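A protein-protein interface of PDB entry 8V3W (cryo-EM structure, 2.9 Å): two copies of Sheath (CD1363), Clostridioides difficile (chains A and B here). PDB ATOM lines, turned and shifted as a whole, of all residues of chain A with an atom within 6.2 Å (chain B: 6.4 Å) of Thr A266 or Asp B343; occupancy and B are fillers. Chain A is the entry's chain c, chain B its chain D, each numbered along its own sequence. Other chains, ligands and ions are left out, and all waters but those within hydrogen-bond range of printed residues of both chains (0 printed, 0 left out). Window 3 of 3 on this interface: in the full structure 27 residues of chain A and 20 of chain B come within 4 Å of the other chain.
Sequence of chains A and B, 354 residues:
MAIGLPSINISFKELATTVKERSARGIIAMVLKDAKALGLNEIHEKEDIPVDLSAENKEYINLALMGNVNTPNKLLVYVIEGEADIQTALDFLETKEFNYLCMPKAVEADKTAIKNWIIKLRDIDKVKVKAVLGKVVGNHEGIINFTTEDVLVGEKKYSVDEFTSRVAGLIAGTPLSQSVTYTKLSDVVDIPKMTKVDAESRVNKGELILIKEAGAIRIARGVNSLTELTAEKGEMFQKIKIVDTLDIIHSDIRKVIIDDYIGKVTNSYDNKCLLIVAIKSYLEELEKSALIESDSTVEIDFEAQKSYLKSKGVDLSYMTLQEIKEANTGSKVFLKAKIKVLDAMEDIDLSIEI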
ATOM      1  N   LYS A 264       9.163 -26.058  18.173  1.00  0.00           N
ATOM      2  CA  LYS A 264      10.371 -26.457  18.878  1.00  0.00           C
ATOM      3  C   LYS A 264      11.448 -27.018  17.966  1.00  0.00           C
ATOM      4  O   LYS A 264      12.576 -27.225  18.425  1.00  0.00           O
ATOM      5  CB  LYS A 264      10.041 -27.510  19.945  1.00  0.00           C
ATOM      6  CG  LYS A 264       9.099 -27.033  21.020  1.00  0.00           C
ATOM      7  CD  LYS A 264       8.885 -28.113  22.059  1.00  0.00           C
ATOM      8  CE  LYS A 264       7.742 -27.755  22.984  1.00  0.00           C
ATOM      9  NZ  LYS A 264       6.439 -27.807  22.276  1.00  0.00           N
ATOM     10  N   VAL A 265      11.138 -27.264  16.699  1.00  0.00           N
ATOM     11  CA  VAL A 265      12.017 -28.005  15.803  1.00  0.00           C
ATOM     12  C   VAL A 265      12.074 -27.279  14.468  1.00  0.00           C
ATOM     13  O   VAL A 265      11.039 -26.863  13.940  1.00  0.00           O
ATOM     14  CB  VAL A 265      11.520 -29.453  15.630  1.00  0.00           C
ATOM     15  CG1 VAL A 265      11.937 -30.011  14.295  1.00  0.00           C
ATOM     16  CG2 VAL A 265      12.036 -30.323  16.756  1.00  0.00           C
ATOM     17  N   THR A 266      13.278 -27.122  13.924  1.00  0.00           N
ATOM     18  CA  THR A 266      13.433 -26.451  12.642  1.00  0.00           C
ATOM     19  C   THR A 266      12.898 -27.321  11.511  1.00  0.00           C
ATOM     20  O   THR A 266      12.925 -28.552  11.576  1.00  0.00           O
ATOM     21  CB  THR A 266      14.899 -26.111  12.380  1.00  0.00           C
ATOM     22  OG1 THR A 266      15.562 -27.254  11.835  1.00  0.00           O
ATOM     23  CG2 THR A 266      15.589 -25.711  13.665  1.00  0.00           C
ATOM     24  N   ASN A 267      12.418 -26.667  10.459  1.00  0.00           N
ATOM     25  CA  ASN A 267      11.755 -27.355   9.354  1.00  0.00           C
ATOM     26  C   ASN A 267      12.794 -27.780   8.327  1.00  0.00           C
ATOM     27  O   ASN A 267      13.066 -27.075   7.357  1.00  0.00           O
ATOM     28  CB  ASN A 267      10.692 -26.463   8.730  1.00  0.00           C
ATOM     29  CG  ASN A 267       9.598 -27.255   8.064  1.00  0.00           C
ATOM     30  OD1 ASN A 267       9.395 -28.425   8.372  1.00  0.00           O
ATOM     31  ND2 ASN A 267       8.896 -26.630   7.134  1.00  0.00           N
ATOM     32  N   SER A 268      13.372 -28.958   8.535  1.00  0.00           N
ATOM     33  CA  SER A 268      14.294 -29.565   7.589  1.00  0.00           C
ATOM     34  C   SER A 268      13.815 -30.974   7.269  1.00  0.00           C
ATOM     35  O   SER A 268      12.896 -31.498   7.901  1.00  0.00           O
ATOM     36  CB  SER A 268      15.728 -29.588   8.133  1.00  0.00           C
ATOM     37  OG  SER A 268      15.842 -30.468   9.235  1.00  0.00           O
ATOM     38  N   ASN A 271      14.148 -33.677  10.161  1.00  0.00           N
ATOM     39  CA  ASN A 271      13.111 -33.609  11.180  1.00  0.00           C
ATOM     40  C   ASN A 271      11.780 -34.133  10.656  1.00  0.00           C
ATOM     41  O   ASN A 271      11.002 -34.721  11.418  1.00  0.00           O
ATOM     42  CB  ASN A 271      12.985 -32.179  11.687  1.00  0.00           C
ATOM     43  CG  ASN A 271      14.241 -31.702  12.390  1.00  0.00           C
ATOM     44  OD1 ASN A 271      14.925 -32.477  13.054  1.00  0.00           O
ATOM     45  ND2 ASN A 271      14.548 -30.422  12.251  1.00  0.00           N
ATOM     46  N   LYS A 272      11.506 -33.947   9.362  1.00  0.00           N
ATOM     47  CA  LYS A 272      10.322 -34.559   8.772  1.00  0.00           C
ATOM     48  C   LYS A 272      10.397 -36.075   8.862  1.00  0.00           C
ATOM     49  O   LYS A 272       9.394 -36.738   9.155  1.00  0.00           O
ATOM     50  CB  LYS A 272      10.166 -34.125   7.317  1.00  0.00           C
ATOM     51  CG  LYS A 272       9.742 -32.685   7.133  1.00  0.00           C
ATOM     52  CD  LYS A 272      10.135 -32.198   5.755  1.00  0.00           C
ATOM     53  CE  LYS A 272      10.035 -30.694   5.642  1.00  0.00           C
ATOM     54  NZ  LYS A 272       8.911 -30.280   4.772  1.00  0.00           N
ATOM     55  N   ASN A 328      13.215 -26.889   0.525  1.00  0.00           N
ATOM     56  CA  ASN A 328      12.722 -26.141   1.672  1.00  0.00           C
ATOM     57  C   ASN A 328      11.311 -25.629   1.408  1.00  0.00           C
ATOM     58  O   ASN A 328      10.993 -25.177   0.306  1.00  0.00           O
ATOM     59  CB  ASN A 328      13.656 -24.974   1.982  1.00  0.00           C
ATOM     60  CG  ASN A 328      13.438 -24.413   3.365  1.00  0.00           C
ATOM     61  OD1 ASN A 328      12.992 -25.119   4.269  1.00  0.00           O
ATOM     62  ND2 ASN A 328      13.746 -23.134   3.542  1.00  0.00           N
ATOM     63  N   GLY A 330       9.458 -23.797   4.190  1.00  0.00           N
ATOM     64  CA  GLY A 330       9.131 -22.656   5.018  1.00  0.00           C
ATOM     65  C   GLY A 330       7.997 -22.885   5.993  1.00  0.00           C
ATOM     66  O   GLY A 330       6.897 -22.353   5.806  1.00  0.00           O
ATOM     67  N   SER A 331       8.245 -23.702   7.015  1.00  0.00           N
ATOM     68  CA  SER A 331       7.347 -23.908   8.148  1.00  0.00           C
ATOM     69  C   SER A 331       6.095 -24.706   7.796  1.00  0.00           C
ATOM     70  O   SER A 331       5.121 -24.681   8.547  1.00  0.00           O
ATOM     71  CB  SER A 331       6.950 -22.575   8.790  1.00  0.00           C
ATOM     72  OG  SER A 331       5.661 -22.651   9.363  1.00  0.00           O
ATOM     73  N   SER B 177      17.082 -21.408  18.882  1.00  0.00           N
ATOM     74  CA  SER B 177      16.602 -22.456  17.989  1.00  0.00           C
ATOM     75  C   SER B 177      15.081 -22.463  17.896  1.00  0.00           C
ATOM     76  O   SER B 177      14.522 -22.738  16.829  1.00  0.00           O
ATOM     77  CB  SER B 177      17.112 -23.814  18.465  1.00  0.00           C
ATOM     78  OG  SER B 177      16.331 -24.865  17.927  1.00  0.00           O
ATOM     79  N   SER B 179      10.892 -21.173  18.723  1.00  0.00           N
ATOM     80  CA  SER B 179       9.989 -20.051  18.533  1.00  0.00           C
ATOM     81  C   SER B 179       8.918 -20.093  19.615  1.00  0.00           C
ATOM     82  O   SER B 179       8.694 -21.126  20.250  1.00  0.00           O
ATOM     83  CB  SER B 179       9.347 -20.075  17.142  1.00  0.00           C
ATOM     84  OG  SER B 179       8.289 -19.144  17.059  1.00  0.00           O
ATOM     85  N   GLU B 235       8.268 -11.263   3.559  1.00  0.00           N
ATOM     86  CA  GLU B 235       7.467 -11.821   4.641  1.00  0.00           C
ATOM     87  C   GLU B 235       8.324 -12.374   5.775  1.00  0.00           C
ATOM     88  O   GLU B 235       7.874 -12.406   6.925  1.00  0.00           O
ATOM     89  CB  GLU B 235       6.538 -12.901   4.083  1.00  0.00           C
ATOM     90  CG  GLU B 235       5.799 -13.722   5.121  1.00  0.00           C
ATOM     91  CD  GLU B 235       6.474 -15.052   5.396  1.00  0.00           C
ATOM     92  OE1 GLU B 235       7.292 -15.488   4.557  1.00  0.00           O
ATOM     93  OE2 GLU B 235       6.189 -15.665   6.447  1.00  0.00           O
ATOM     94  N   LYS B 239       8.583 -12.394  11.390  1.00  0.00           N
ATOM     95  CA  LYS B 239       8.759 -13.390  12.436  1.00  0.00           C
ATOM     96  C   LYS B 239       9.732 -12.878  13.487  1.00  0.00           C
ATOM     97  O   LYS B 239      10.738 -12.243  13.160  1.00  0.00           O
ATOM     98  CB  LYS B 239       9.264 -14.709  11.848  1.00  0.00           C
ATOM     99  CG  LYS B 239       8.582 -15.110  10.554  1.00  0.00           C
ATOM    100  CD  LYS B 239       7.136 -15.489  10.802  1.00  0.00           C
ATOM    101  CE  LYS B 239       7.048 -16.838  11.486  1.00  0.00           C
ATOM    102  NZ  LYS B 239       5.844 -16.949  12.346  1.00  0.00           N
ATOM    103  N   LYS B 241      11.621 -14.702  15.551  1.00  0.00           N
ATOM    104  CA  LYS B 241      12.852 -15.486  15.601  1.00  0.00           C
ATOM    105  C   LYS B 241      13.859 -15.021  14.551  1.00  0.00           C
ATOM    106  O   LYS B 241      15.061 -14.896  14.837  1.00  0.00           O
ATOM    107  CB  LYS B 241      12.500 -16.963  15.426  1.00  0.00           C
ATOM    108  CG  LYS B 241      13.637 -17.873  15.042  1.00  0.00           C
ATOM    109  CD  LYS B 241      13.146 -19.306  14.953  1.00  0.00           C
ATOM    110  CE  LYS B 241      13.951 -20.103  13.954  1.00  0.00           C
ATOM    111  NZ  LYS B 241      15.368 -20.224  14.370  1.00  0.00           N
ATOM    112  N   ILE B 242      13.384 -14.749  13.334  1.00  0.00           N
ATOM    113  CA  ILE B 242      14.270 -14.308  12.258  1.00  0.00           C
ATOM    114  C   ILE B 242      14.887 -12.958  12.595  1.00  0.00           C
ATOM    115  O   ILE B 242      16.091 -12.740  12.413  1.00  0.00           O
ATOM    116  CB  ILE B 242      13.509 -14.261  10.923  1.00  0.00           C
ATOM    117  CG1 ILE B 242      12.716 -15.547  10.713  1.00  0.00           C
ATOM    118  CG2 ILE B 242      14.465 -14.024   9.772  1.00  0.00           C
ATOM    119  CD1 ILE B 242      13.570 -16.770  10.582  1.00  0.00           C
ATOM    120  N   VAL B 341      18.792 -18.536   6.488  1.00  0.00           N
ATOM    121  CA  VAL B 341      18.277 -18.888   7.807  1.00  0.00           C
ATOM    122  C   VAL B 341      16.994 -19.691   7.637  1.00  0.00           C
ATOM    123  O   VAL B 341      16.229 -19.478   6.692  1.00  0.00           O
ATOM    124  CB  VAL B 341      18.026 -17.636   8.678  1.00  0.00           C
ATOM    125  CG1 VAL B 341      17.632 -18.029  10.087  1.00  0.00           C
ATOM    126  CG2 VAL B 341      19.255 -16.747   8.709  1.00  0.00           C
ATOM    127  N   LEU B 342      16.761 -20.620   8.561  1.00  0.00           N
ATOM    128  CA  LEU B 342      15.608 -21.508   8.527  1.00  0.00           C
ATOM    129  C   LEU B 342      14.539 -21.062   9.521  1.00  0.00           C
ATOM    130  O   LEU B 342      14.760 -20.202  10.375  1.00  0.00           O
ATOM    131  CB  LEU B 342      16.035 -22.946   8.829  1.00  0.00           C
ATOM    132  CG  LEU B 342      16.810 -23.696   7.749  1.00  0.00           C
ATOM    133  CD1 LEU B 342      16.917 -25.169   8.106  1.00  0.00           C
ATOM    134  CD2 LEU B 342      16.158 -23.513   6.393  1.00  0.00           C
ATOM    135  N   ASP B 343      13.363 -21.677   9.404  1.00  0.00           N
ATOM    136  CA  ASP B 343      12.241 -21.413  10.290  1.00  0.00           C
ATOM    137  C   ASP B 343      11.735 -22.724  10.872  1.00  0.00           C
ATOM    138  O   ASP B 343      11.947 -23.800  10.309  1.00  0.00           O
ATOM    139  CB  ASP B 343      11.102 -20.689   9.563  1.00  0.00           C
ATOM    140  CG  ASP B 343      10.189 -19.939  10.516  1.00  0.00           C
ATOM    141  OD1 ASP B 343      10.351 -20.097  11.743  1.00  0.00           O
ATOM    142  OD2 ASP B 343       9.305 -19.198  10.041  1.00  0.00           O
ATOM    143  N   ALA B 344      11.064 -22.624  12.016  1.00  0.00           N
ATOM    144  CA  ALA B 344      10.594 -23.798  12.732  1.00  0.00           C
ATOM    145  C   ALA B 344       9.267 -24.294  12.165  1.00  0.00           C
ATOM    146  O   ALA B 344       8.582 -23.596  11.415  1.00  0.00           O
ATOM    147  CB  ALA B 344      10.446 -23.493  14.220  1.00  0.00           C
ATOM    148  N   MET B 345       8.912 -25.525  12.534  1.00  0.00           N
ATOM    149  CA  MET B 345       7.652 -26.111  12.093  1.00  0.00           C
ATOM    150  C   MET B 345       6.474 -25.411  12.752  1.00  0.00           C
ATOM    151  O   MET B 345       6.450 -25.234  13.972  1.00  0.00           O
ATOM    152  CB  MET B 345       7.607 -27.600  12.426  1.00  0.00           C
ATOM    153  CG  MET B 345       8.631 -28.453  11.729  1.00  0.00           C
ATOM    154  SD  MET B 345       8.320 -30.197  12.057  1.00  0.00           S
ATOM    155  CE  MET B 345       9.689 -30.947  11.201  1.00  0.00           C
ATOM    156  N   GLU B 346       5.493 -25.013  11.944  1.00  0.00           N
ATOM    157  CA  GLU B 346       4.295 -24.387  12.484  1.00  0.00           C
ATOM    158  C   GLU B 346       2.996 -24.821  11.822  1.00  0.00           C
ATOM    159  O   GLU B 346       1.933 -24.536  12.378  1.00  0.00           O
ATOM    160  CB  GLU B 346       4.420 -22.861  12.401  1.00  0.00           C
ATOM    161  CG  GLU B 346       5.326 -22.281  13.473  1.00  0.00           C
ATOM    162  CD  GLU B 346       5.789 -20.878  13.161  1.00  0.00           C
ATOM    163  OE1 GLU B 346       5.393 -20.335  12.111  1.00  0.00           O
ATOM    164  OE2 GLU B 346       6.554 -20.316  13.968  1.00  0.00           O
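The backbone NH of Met B345 lies within hydrogen-bond range of the backbone carbonyl oxygen of Val A265.
The backbone NH (N) of Asn A267 lies within hydrogen-bond range of the backbone carbonyl oxygen (O) of Asp B343 (2.9 Å).
The backbone NH (N) of Glu B346 lies within hydrogen-bond range of the backbone carbonyl oxygen (O) of Ser A331 (3.4 Å).
The backbone carbonyl oxygen of Thr A266 is in hydrogen-bond range of the side-chain amide nitrogen of Asn A271 (2.6 Å).
The side-chain amide nitrogen of Asn A267 lies close to the backbone NH of Ser A331.
The side-chain hydroxyl (OG) of Ser A268 sits at hydrogen-bond distance from the side-chain amide nitrogen (ND2) of Asn A271, 3.3 Å away.
The side-chain amino group of Lys B239 lies within salt-bridge range of the side-chain carboxylate of Glu B346, 3.4 Å away.
Ala B344 touches Val A265.
CA of Thr A266 touches O of Asp B343 (3.8 Å).
Thr A266 touches Ala B344.
Met B345 touches Asn A267 (CG to OD1, 3.4 Å).
Asn A271 touches Met B345.
N of Lys A272 touches CE of Met B345, 3.96 Å away.
ND2 of Asn A328 touches CD2 of Leu B342, at 3.8 Å.
Ser A331 touches Ala B344 (CB to O, 3.3 Å).
Of the printed residues of chain B, Thr A266 touches Asp B343 and Ala B344.
Of the printed residues of chain B, Asn A271 touches Met B345.
Of the printed residues of chain B, Ser A331 touches Ala B344 and Glu B346.
Val B341 touches none of the printed residues of chain A.
Of the printed residues of chain A, Leu B342 touches Asn A328 (3.8 Å).
Asp B343 touches just these residues of chain A: Thr A266 and Asn A267.
Of the printed residues of chain A, Ala B344 touches Val A265, Thr A266 and Ser A331.
Printed residues of chain A within 4 Å of Met B345: Val A265 (2.9 Å), Asn A267 (3.4 Å), Asn A271 (3.6 Å) and Lys A272 (3.96 Å).
The nearest residue of chain B that does not touch Thr A266 is Met B345 (4.04 Å).
The nearest residue of chain A that does not touch Asp B343 is Ser A331 (4.3 Å).
The nearest printed residue of chain A that does not touch Met B345 is Thr A266 (4.04 Å).
Printed residues of chain A that touch a printed residue of chain B: Val A265, Thr A266, Asn A267, Asn A271, Lys A272, Asn A328 and Ser A331.
Hydrophobic or aromatic side chains of chain A within 4 Å of the printed part of chain B: Val A265.
Hydrophobic or aromatic side chains of chain B within 4 Å of the printed part of chain A: Leu B342, Ala B344 and Met B345.
Among the printed residues, no Asp or Glu carboxylate lies within 4 Å of a Lys or Arg side-chain nitrogen of the other chain.
No position is printed for both chains.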
